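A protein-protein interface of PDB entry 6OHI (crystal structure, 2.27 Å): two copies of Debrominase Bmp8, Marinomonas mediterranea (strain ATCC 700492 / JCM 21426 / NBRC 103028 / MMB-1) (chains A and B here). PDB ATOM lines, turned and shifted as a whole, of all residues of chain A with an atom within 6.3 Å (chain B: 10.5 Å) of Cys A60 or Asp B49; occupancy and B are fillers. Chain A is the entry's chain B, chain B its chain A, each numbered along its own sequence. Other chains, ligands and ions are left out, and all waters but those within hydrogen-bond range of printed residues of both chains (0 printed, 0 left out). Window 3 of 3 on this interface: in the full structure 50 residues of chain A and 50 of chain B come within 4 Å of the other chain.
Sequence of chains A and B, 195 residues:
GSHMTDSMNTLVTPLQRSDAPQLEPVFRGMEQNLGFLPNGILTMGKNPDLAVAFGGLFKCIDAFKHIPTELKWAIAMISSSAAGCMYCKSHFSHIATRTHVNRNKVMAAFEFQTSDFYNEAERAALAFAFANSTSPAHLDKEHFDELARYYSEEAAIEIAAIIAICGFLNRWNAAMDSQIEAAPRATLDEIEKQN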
ATOM      1  N   GLY A  55      18.773   2.999   1.430  1.00  0.00           N
ATOM      2  CA  GLY A  55      17.480   2.575   0.902  1.00  0.00           C
ATOM      3  C   GLY A  55      16.824   3.683   0.100  1.00  0.00           C
ATOM      4  O   GLY A  55      16.307   3.444  -0.975  1.00  0.00           O
ATOM      5  N   GLY A  56      16.854   4.899   0.658  1.00  0.00           N
ATOM      6  CA  GLY A  56      16.388   6.111   0.010  1.00  0.00           C
ATOM      7  C   GLY A  56      17.061   6.350  -1.334  1.00  0.00           C
ATOM      8  O   GLY A  56      16.396   6.704  -2.318  1.00  0.00           O
ATOM      9  N   LEU A  57      18.385   6.156  -1.379  1.00  0.00           N
ATOM     10  CA  LEU A  57      19.150   6.332  -2.609  1.00  0.00           C
ATOM     11  C   LEU A  57      18.735   5.277  -3.642  1.00  0.00           C
ATOM     12  O   LEU A  57      18.514   5.605  -4.808  1.00  0.00           O
ATOM     13  CB  LEU A  57      20.645   6.233  -2.300  1.00  0.00           C
ATOM     14  CG  LEU A  57      21.567   6.415  -3.504  1.00  0.00           C
ATOM     15  CD1 LEU A  57      21.332   7.760  -4.166  1.00  0.00           C
ATOM     16  CD2 LEU A  57      23.021   6.265  -3.089  1.00  0.00           C
ATOM     17  N   PHE A  58      18.620   4.020  -3.203  1.00  0.00           N
ATOM     18  CA  PHE A  58      18.374   2.916  -4.117  1.00  0.00           C
ATOM     19  C   PHE A  58      16.993   3.028  -4.787  1.00  0.00           C
ATOM     20  O   PHE A  58      16.845   2.644  -5.967  1.00  0.00           O
ATOM     21  CB  PHE A  58      18.505   1.567  -3.413  1.00  0.00           C
ATOM     22  CG  PHE A  58      18.386   0.405  -4.364  1.00  0.00           C
ATOM     23  CD1 PHE A  58      19.480  -0.035  -5.092  1.00  0.00           C
ATOM     24  CD2 PHE A  58      17.162  -0.215  -4.571  1.00  0.00           C
ATOM     25  CE1 PHE A  58      19.361  -1.093  -5.980  1.00  0.00           C
ATOM     26  CE2 PHE A  58      17.049  -1.274  -5.457  1.00  0.00           C
ATOM     27  CZ  PHE A  58      18.148  -1.707  -6.164  1.00  0.00           C
ATOM     28  N   LYS A  59      15.996   3.525  -4.045  1.00  0.00           N
ATOM     29  CA  LYS A  59      14.628   3.640  -4.561  1.00  0.00           C
ATOM     30  C   LYS A  59      14.572   4.685  -5.686  1.00  0.00           C
ATOM     31  O   LYS A  59      13.659   4.629  -6.492  1.00  0.00           O
ATOM     32  CB  LYS A  59      13.620   3.962  -3.446  1.00  0.00           C
ATOM     33  CG  LYS A  59      13.692   5.374  -2.880  1.00  0.00           C
ATOM     34  CD  LYS A  59      12.373   5.988  -2.431  1.00  0.00           C
ATOM     35  CE  LYS A  59      12.512   7.474  -2.155  1.00  0.00           C
ATOM     36  NZ  LYS A  59      11.446   7.981  -1.256  1.00  0.00           N
ATOM     37  N   CYS A  60      15.552   5.602  -5.750  1.00  0.00           N
ATOM     38  CA  CYS A  60      15.640   6.611  -6.825  1.00  0.00           C
ATOM     39  C   CYS A  60      15.655   5.943  -8.208  1.00  0.00           C
ATOM     40  O   CYS A  60      15.186   6.538  -9.183  1.00  0.00           O
ATOM     41  CB  CYS A  60      16.880   7.492  -6.717  1.00  0.00           C
ATOM     42  SG  CYS A  60      16.801   8.750  -5.415  1.00  0.00           S
ATOM     43  N   ILE A  61      16.190   4.719  -8.298  1.00  0.00           N
ATOM     44  CA  ILE A  61      16.298   4.026  -9.588  1.00  0.00           C
ATOM     45  C   ILE A  61      14.900   3.825 -10.190  1.00  0.00           C
ATOM     46  O   ILE A  61      14.666   4.209 -11.330  1.00  0.00           O
ATOM     47  CB  ILE A  61      17.064   2.697  -9.451  1.00  0.00           C
ATOM     48  CG1 ILE A  61      18.508   2.946  -9.007  1.00  0.00           C
ATOM     49  CG2 ILE A  61      16.994   1.884 -10.744  1.00  0.00           C
ATOM     50  CD1 ILE A  61      19.383   1.710  -8.989  1.00  0.00           C
ATOM     51  N   ASP A  62      13.983   3.222  -9.421  1.00  0.00           N
ATOM     52  CA  ASP A  62      12.634   2.916  -9.909  1.00  0.00           C
ATOM     53  C   ASP A  62      11.891   4.218 -10.239  1.00  0.00           C
ATOM     54  O   ASP A  62      11.084   4.241 -11.149  1.00  0.00           O
ATOM     55  CB  ASP A  62      11.849   2.051  -8.914  1.00  0.00           C
ATOM     56  CG  ASP A  62      11.968   0.554  -9.171  1.00  0.00           C
ATOM     57  OD1 ASP A  62      11.953   0.156 -10.354  1.00  0.00           O
ATOM     58  OD2 ASP A  62      12.071  -0.209  -8.187  1.00  0.00           O
ATOM     59  N   ALA A  63      12.192   5.297  -9.510  1.00  0.00           N
ATOM     60  CA  ALA A  63      11.505   6.590  -9.651  1.00  0.00           C
ATOM     61  C   ALA A  63      11.986   7.375 -10.887  1.00  0.00           C
ATOM     62  O   ALA A  63      11.282   8.275 -11.342  1.00  0.00           O
ATOM     63  CB  ALA A  63      11.693   7.400  -8.387  1.00  0.00           C
ATOM     64  N   PHE A  64      13.172   7.061 -11.425  1.00  0.00           N
ATOM     65  CA  PHE A  64      13.715   7.790 -12.598  1.00  0.00           C
ATOM     66  C   PHE A  64      12.748   7.675 -13.783  1.00  0.00           C
ATOM     67  O   PHE A  64      12.170   6.621 -14.004  1.00  0.00           O
ATOM     68  CB  PHE A  64      15.106   7.274 -12.974  1.00  0.00           C
ATOM     69  CG  PHE A  64      16.210   7.646 -12.014  1.00  0.00           C
ATOM     70  CD1 PHE A  64      16.209   8.860 -11.342  1.00  0.00           C
ATOM     71  CD2 PHE A  64      17.258   6.770 -11.779  1.00  0.00           C
ATOM     72  CE1 PHE A  64      17.227   9.184 -10.458  1.00  0.00           C
ATOM     73  CE2 PHE A  64      18.278   7.100 -10.902  1.00  0.00           C
ATOM     74  CZ  PHE A  64      18.262   8.306 -10.244  1.00  0.00           C
ATOM     75  N   LYS A  72      17.571   0.818 -17.442  1.00  0.00           N
ATOM     76  CA  LYS A  72      17.987   0.998 -16.051  1.00  0.00           C
ATOM     77  C   LYS A  72      18.781  -0.224 -15.572  1.00  0.00           C
ATOM     78  O   LYS A  72      19.882  -0.075 -15.051  1.00  0.00           O
ATOM     79  CB  LYS A  72      16.783   1.229 -15.133  1.00  0.00           C
ATOM     80  CG  LYS A  72      16.066   2.561 -15.321  1.00  0.00           C
ATOM     81  CD  LYS A  72      14.868   2.701 -14.408  1.00  0.00           C
ATOM     82  CE  LYS A  72      14.014   3.912 -14.703  1.00  0.00           C
ATOM     83  NZ  LYS A  72      13.040   4.154 -13.613  1.00  0.00           N
ATOM     84  N   ILE A 165      25.232   4.413  -8.035  1.00  0.00           N
ATOM     85  CA  ILE A 165      24.582   3.555  -7.038  1.00  0.00           C
ATOM     86  C   ILE A 165      25.194   2.150  -7.091  1.00  0.00           C
ATOM     87  O   ILE A 165      25.351   1.503  -6.063  1.00  0.00           O
ATOM     88  CB  ILE A 165      23.053   3.538  -7.229  1.00  0.00           C
ATOM     89  CG1 ILE A 165      22.453   4.907  -6.908  1.00  0.00           C
ATOM     90  CG2 ILE A 165      22.421   2.443  -6.386  1.00  0.00           C
ATOM     91  CD1 ILE A 165      21.036   5.093  -7.378  1.00  0.00           C
ATOM     92  N   ALA B  20      18.761  26.577  -6.175  1.00  0.00           N
ATOM     93  CA  ALA B  20      18.249  25.446  -5.388  1.00  0.00           C
ATOM     94  C   ALA B  20      18.548  25.646  -3.905  1.00  0.00           C
ATOM     95  O   ALA B  20      19.433  25.002  -3.344  1.00  0.00           O
ATOM     96  CB  ALA B  20      18.835  24.153  -5.905  1.00  0.00           C
ATOM     97  N   GLN B  22      16.624  24.731  -1.482  1.00  0.00           N
ATOM     98  CA  GLN B  22      16.087  23.574  -0.751  1.00  0.00           C
ATOM     99  C   GLN B  22      17.199  22.553  -0.463  1.00  0.00           C
ATOM    100  O   GLN B  22      17.081  21.741   0.465  1.00  0.00           O
ATOM    101  CB  GLN B  22      14.924  22.917  -1.499  1.00  0.00           C
ATOM    102  CG  GLN B  22      15.252  22.398  -2.893  1.00  0.00           C
ATOM    103  CD  GLN B  22      14.009  21.806  -3.520  1.00  0.00           C
ATOM    104  OE1 GLN B  22      13.300  21.029  -2.891  1.00  0.00           O
ATOM    105  NE2 GLN B  22      13.715  22.184  -4.756  1.00  0.00           N
ATOM    106  N   LEU B  23      18.279  22.607  -1.249  1.00  0.00           N
ATOM    107  CA  LEU B  23      19.364  21.641  -1.136  1.00  0.00           C
ATOM    108  C   LEU B  23      20.459  22.130  -0.172  1.00  0.00           C
ATOM    109  O   LEU B  23      21.438  21.426   0.027  1.00  0.00           O
ATOM    110  CB  LEU B  23      19.921  21.370  -2.537  1.00  0.00           C
ATOM    111  CG  LEU B  23      18.921  20.776  -3.530  1.00  0.00           C
ATOM    112  CD1 LEU B  23      19.537  20.632  -4.917  1.00  0.00           C
ATOM    113  CD2 LEU B  23      18.387  19.437  -3.029  1.00  0.00           C
ATOM    114  N   VAL B  26      21.911  19.762   2.236  1.00  0.00           N
ATOM    115  CA  VAL B  26      22.776  18.771   1.562  1.00  0.00           C
ATOM    116  C   VAL B  26      24.147  19.396   1.249  1.00  0.00           C
ATOM    117  O   VAL B  26      25.182  18.768   1.483  1.00  0.00           O
ATOM    118  CB  VAL B  26      22.106  18.232   0.280  1.00  0.00           C
ATOM    119  CG1 VAL B  26      23.054  17.368  -0.551  1.00  0.00           C
ATOM    120  CG2 VAL B  26      20.818  17.486   0.601  1.00  0.00           C
ATOM    121  N   ILE B  41      27.967  18.329  -7.099  1.00  0.00           N
ATOM    122  CA  ILE B  41      26.787  18.262  -6.261  1.00  0.00           C
ATOM    123  C   ILE B  41      25.723  19.226  -6.800  1.00  0.00           C
ATOM    124  O   ILE B  41      24.531  18.949  -6.697  1.00  0.00           O
ATOM    125  CB  ILE B  41      27.132  18.546  -4.786  1.00  0.00           C
ATOM    126  CG1 ILE B  41      28.252  17.630  -4.278  1.00  0.00           C
ATOM    127  CG2 ILE B  41      25.878  18.450  -3.929  1.00  0.00           C
ATOM    128  CD1 ILE B  41      27.931  16.143  -4.345  1.00  0.00           C
ATOM    129  N   THR B  43      25.406  19.810  -9.988  1.00  0.00           N
ATOM    130  CA  THR B  43      24.862  19.075 -11.150  1.00  0.00           C
ATOM    131  C   THR B  43      23.824  18.061 -10.650  1.00  0.00           C
ATOM    132  O   THR B  43      22.748  17.929 -11.234  1.00  0.00           O
ATOM    133  CB  THR B  43      25.952  18.385 -11.981  1.00  0.00           C
ATOM    134  OG1 THR B  43      26.707  17.537 -11.119  1.00  0.00           O
ATOM    135  CG2 THR B  43      26.908  19.343 -12.656  1.00  0.00           C
ATOM    136  N   MET B  44      24.154  17.380  -9.545  1.00  0.00           N
ATOM    137  CA  MET B  44      23.269  16.385  -8.915  1.00  0.00           C
ATOM    138  C   MET B  44      21.942  17.037  -8.505  1.00  0.00           C
ATOM    139  O   MET B  44      20.918  16.374  -8.466  1.00  0.00           O
ATOM    140  CB  MET B  44      23.933  15.793  -7.672  1.00  0.00           C
ATOM    141  CG  MET B  44      23.375  14.466  -7.259  1.00  0.00           C
ATOM    142  SD  MET B  44      24.217  13.796  -5.796  1.00  0.00           S
ATOM    143  CE  MET B  44      25.894  13.635  -6.417  1.00  0.00           C
ATOM    144  N   GLY B  45      21.999  18.341  -8.208  1.00  0.00           N
ATOM    145  CA  GLY B  45      20.867  19.148  -7.759  1.00  0.00           C
ATOM    146  C   GLY B  45      19.696  19.167  -8.727  1.00  0.00           C
ATOM    147  O   GLY B  45      18.536  19.318  -8.300  1.00  0.00           O
ATOM    148  N   LYS B  46      19.985  18.980 -10.018  1.00  0.00           N
ATOM    149  CA  LYS B  46      18.976  19.041 -11.075  1.00  0.00           C
ATOM    150  C   LYS B  46      18.021  17.840 -11.004  1.00  0.00           C
ATOM    151  O   LYS B  46      17.003  17.822 -11.699  1.00  0.00           O
ATOM    152  CB  LYS B  46      19.652  19.118 -12.446  1.00  0.00           C
ATOM    153  CG  LYS B  46      20.377  20.425 -12.722  1.00  0.00           C
ATOM    154  CD  LYS B  46      20.719  20.630 -14.184  1.00  0.00           C
ATOM    155  CE  LYS B  46      21.222  22.027 -14.473  1.00  0.00           C
ATOM    156  NZ  LYS B  46      21.677  22.159 -15.877  1.00  0.00           N
ATOM    157  N   ASN B  47      18.369  16.835 -10.195  1.00  0.00           N
ATOM    158  CA  ASN B  47      17.474  15.739  -9.888  1.00  0.00           C
ATOM    159  C   ASN B  47      17.263  15.730  -8.377  1.00  0.00           C
ATOM    160  O   ASN B  47      18.021  15.095  -7.647  1.00  0.00           O
ATOM    161  CB  ASN B  47      17.998  14.419 -10.450  1.00  0.00           C
ATOM    162  CG  ASN B  47      17.035  13.275 -10.247  1.00  0.00           C
ATOM    163  OD1 ASN B  47      16.496  13.103  -9.162  1.00  0.00           O
ATOM    164  ND2 ASN B  47      16.810  12.495 -11.287  1.00  0.00           N
ATOM    165  N   PRO B  48      16.240  16.454  -7.864  1.00  0.00           N
ATOM    166  CA  PRO B  48      16.098  16.692  -6.430  1.00  0.00           C
ATOM    167  C   PRO B  48      16.056  15.409  -5.588  1.00  0.00           C
ATOM    168  O   PRO B  48      16.642  15.392  -4.506  1.00  0.00           O
ATOM    169  CB  PRO B  48      14.769  17.456  -6.309  1.00  0.00           C
ATOM    170  CG  PRO B  48      14.554  18.072  -7.678  1.00  0.00           C
ATOM    171  CD  PRO B  48      15.178  17.097  -8.652  1.00  0.00           C
ATOM    172  N   ASP B  49      15.375  14.367  -6.091  1.00  0.00           N
ATOM    173  CA  ASP B  49      15.292  13.056  -5.435  1.00  0.00           C
ATOM    174  C   ASP B  49      16.691  12.482  -5.187  1.00  0.00           C
ATOM    175  O   ASP B  49      16.949  11.922  -4.130  1.00  0.00           O
ATOM    176  CB  ASP B  49      14.504  12.046  -6.274  1.00  0.00           C
ATOM    177  CG  ASP B  49      13.010  12.065  -6.032  1.00  0.00           C
ATOM    178  OD1 ASP B  49      12.538  13.052  -5.460  1.00  0.00           O
ATOM    179  OD2 ASP B  49      12.343  11.079  -6.401  1.00  0.00           O
ATOM    180  N   LEU B  50      17.564  12.614  -6.190  1.00  0.00           N
ATOM    181  CA  LEU B  50      18.896  12.059  -6.154  1.00  0.00           C
ATOM    182  C   LEU B  50      19.750  12.826  -5.146  1.00  0.00           C
ATOM    183  O   LEU B  50      20.405  12.225  -4.295  1.00  0.00           O
ATOM    184  CB  LEU B  50      19.511  12.143  -7.553  1.00  0.00           C
ATOM    185  CG  LEU B  50      20.936  11.608  -7.657  1.00  0.00           C
ATOM    186  CD1 LEU B  50      21.004  10.135  -7.281  1.00  0.00           C
ATOM    187  CD2 LEU B  50      21.471  11.826  -9.061  1.00  0.00           C
ATOM    188  N   ALA B  51      19.728  14.155  -5.261  1.00  0.00           N
ATOM    189  CA  ALA B  51      20.540  15.029  -4.431  1.00  0.00           C
ATOM    190  C   ALA B  51      20.200  14.834  -2.951  1.00  0.00           C
ATOM    191  O   ALA B  51      21.107  14.707  -2.119  1.00  0.00           O
ATOM    192  CB  ALA B  51      20.321  16.456  -4.845  1.00  0.00           C
ATOM    193  N   VAL B  52      18.898  14.815  -2.625  1.00  0.00           N
ATOM    194  CA  VAL B  52      18.446  14.663  -1.231  1.00  0.00           C
ATOM    195  C   VAL B  52      18.882  13.287  -0.715  1.00  0.00           C
ATOM    196  O   VAL B  52      19.396  13.185   0.395  1.00  0.00           O
ATOM    197  CB  VAL B  52      16.920  14.866  -1.074  1.00  0.00           C
ATOM    198  CG1 VAL B  52      16.377  14.236   0.207  1.00  0.00           C
ATOM    199  CG2 VAL B  52      16.530  16.334  -1.150  1.00  0.00           C
ATOM    200  N   ALA B  53      18.653  12.237  -1.513  1.00  0.00           N
ATOM    201  CA  ALA B  53      18.984  10.859  -1.098  1.00  0.00           C
ATOM    202  C   ALA B  53      20.500  10.724  -0.926  1.00  0.00           C
ATOM    203  O   ALA B  53      20.959  10.238   0.093  1.00  0.00           O
ATOM    204  CB  ALA B  53      18.450   9.854  -2.086  1.00  0.00           C
ATOM    205  N   PHE B  54      21.276  11.192  -1.907  1.00  0.00           N
ATOM    206  CA  PHE B  54      22.710  11.068  -1.785  1.00  0.00           C
ATOM    207  C   PHE B  54      23.234  11.931  -0.629  1.00  0.00           C
ATOM    208  O   PHE B  54      24.131  11.507   0.103  1.00  0.00           O
ATOM    209  CB  PHE B  54      23.462  11.436  -3.058  1.00  0.00           C
ATOM    210  CG  PHE B  54      24.941  11.368  -2.805  1.00  0.00           C
ATOM    211  CD1 PHE B  54      25.563  10.142  -2.636  1.00  0.00           C
ATOM    212  CD2 PHE B  54      25.679  12.517  -2.599  1.00  0.00           C
ATOM    213  CE1 PHE B  54      26.913  10.069  -2.332  1.00  0.00           C
ATOM    214  CE2 PHE B  54      27.027  12.441  -2.292  1.00  0.00           C
ATOM    215  CZ  PHE B  54      27.641  11.224  -2.156  1.00  0.00           C
ATOM    216  N   GLY B  55      22.686  13.137  -0.479  1.00  0.00           N
ATOM    217  CA  GLY B  55      23.049  14.043   0.621  1.00  0.00           C
ATOM    218  C   GLY B  55      22.872  13.383   1.974  1.00  0.00           C
ATOM    219  O   GLY B  55      23.754  13.459   2.830  1.00  0.00           O
ATOM    220  N   GLY B  56      21.717  12.727   2.140  1.00  0.00           N
ATOM    221  CA  GLY B  56      21.388  11.944   3.321  1.00  0.00           C
ATOM    222  C   GLY B  56      22.411  10.852   3.594  1.00  0.00           C
ATOM    223  O   GLY B  56      22.804  10.625   4.731  1.00  0.00           O
ATOM    224  N   LEU B  57      22.847  10.170   2.538  1.00  0.00           N
ATOM    225  CA  LEU B  57      23.821   9.098   2.655  1.00  0.00           C
ATOM    226  C   LEU B  57      25.175   9.670   3.079  1.00  0.00           C
ATOM    227  O   LEU B  57      25.814   9.132   3.969  1.00  0.00           O
ATOM    228  CB  LEU B  57      23.922   8.369   1.314  1.00  0.00           C
ATOM    229  CG  LEU B  57      24.885   7.195   1.267  1.00  0.00           C
ATOM    230  CD1 LEU B  57      24.537   6.172   2.333  1.00  0.00           C
ATOM    231  CD2 LEU B  57      24.872   6.564  -0.109  1.00  0.00           C
ATOM    232  N   PHE B 168      30.195   5.539  -4.901  1.00  0.00           N
ATOM    233  CA  PHE B 168      29.253   6.426  -5.548  1.00  0.00           C
ATOM    234  C   PHE B 168      29.996   7.652  -6.099  1.00  0.00           C
ATOM    235  O   PHE B 168      29.832   8.004  -7.263  1.00  0.00           O
ATOM    236  CB  PHE B 168      28.124   6.805  -4.586  1.00  0.00           C
ATOM    237  CG  PHE B 168      27.089   7.711  -5.202  1.00  0.00           C
ATOM    238  CD1 PHE B 168      27.327   9.069  -5.329  1.00  0.00           C
ATOM    239  CD2 PHE B 168      25.906   7.202  -5.693  1.00  0.00           C
ATOM    240  CE1 PHE B 168      26.398   9.904  -5.927  1.00  0.00           C
ATOM    241  CE2 PHE B 168      24.970   8.038  -6.288  1.00  0.00           C
ATOM    242  CZ  PHE B 168      25.215   9.387  -6.407  1.00  0.00           C
ATOM    243  N   TRP B 172      30.502   8.945  -9.868  1.00  0.00           N
ATOM    244  CA  TRP B 172      29.752  10.167 -10.155  1.00  0.00           C
ATOM    245  C   TRP B 172      30.680  11.259 -10.718  1.00  0.00           C
ATOM    246  O   TRP B 172      30.378  11.875 -11.732  1.00  0.00           O
ATOM    247  CB  TRP B 172      28.985  10.651  -8.925  1.00  0.00           C
ATOM    248  CG  TRP B 172      28.235  11.910  -9.202  1.00  0.00           C
ATOM    249  CD1 TRP B 172      28.639  13.178  -8.901  1.00  0.00           C
ATOM    250  CD2 TRP B 172      26.985  12.033  -9.905  1.00  0.00           C
ATOM    251  NE1 TRP B 172      27.722  14.077  -9.366  1.00  0.00           N
ATOM    252  CE2 TRP B 172      26.689  13.410  -9.971  1.00  0.00           C
ATOM    253  CE3 TRP B 172      26.092  11.126 -10.483  1.00  0.00           C
ATOM    254  CZ2 TRP B 172      25.531  13.898 -10.573  1.00  0.00           C
ATOM    255  CZ3 TRP B 172      24.949  11.607 -11.082  1.00  0.00           C
ATOM    256  CH2 TRP B 172      24.680  12.976 -11.137  1.00  0.00           C
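The side-chain sulfur (SG) of Cys A60 is in hydrogen-bond range of the backbone carbonyl oxygen (O) of Asp B49 (3.4 Å).
The backbone carbonyl oxygen (O) of Gly A56 is in hydrogen-bond range of the side-chain sulfur (SG) of Cys A60. OD1 of Asn B47 lies within hydrogen-bond range of N of Leu B50. NZ of Lys A72 is in hydrogen-bond range of O of Phe A64, at 2.6 Å. O of Leu A57 sits close to SG of Cys A60, 3.6 Å away.
Among the printed residues, merely in contact across the chains: Gly A56 with Ala B53, Leu A57 with Leu B50, Leu A57 with Ala B53, Leu A57 with Leu B57, Leu A57 with Phe B168, Cys A60 with Leu B50, Cys A60 with Ala B53, Phe A64 with Asn B47 and Ile A165 with Phe B168.
Printed residues of chain B within 4 Å of Cys A60: Asp B49, Leu B50 and Ala B53. Printed residues of chain A within 4 Å of Asp B49: Cys A60. Of chain B, only Asn B47 (3.4 Å) comes within 4 Å of Phe A64. Printed residues of chain A within 4 Å of Phe B168: Leu A57 and Ile A165. Of the printed residues of chain B, Leu A57 touches Leu B50 (3.9 Å), Ala B53 (3.6 Å), Leu B57 (3.5 Å) and Phe B168 (3.998 Å). Of the printed residues of chain A, Leu B57 touches Leu A57. Lys B46 touches none of the printed residues of chain A. Trp B172 touches none of the printed residues of chain A. The nearest printed residue of chain A that does not touch Asn B47 is Cys A60 (5.8 Å).
Among the printed residues, no Asp or Glu carboxylate lies within 4 Å of a Lys or Arg side-chain nitrogen of the other chain.
Leu B57 touches its own counterpart, Leu A57. Of the 10 pairs that touch across the chains among the printed residues, 1 has its exchanged pair printed and touching as well.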
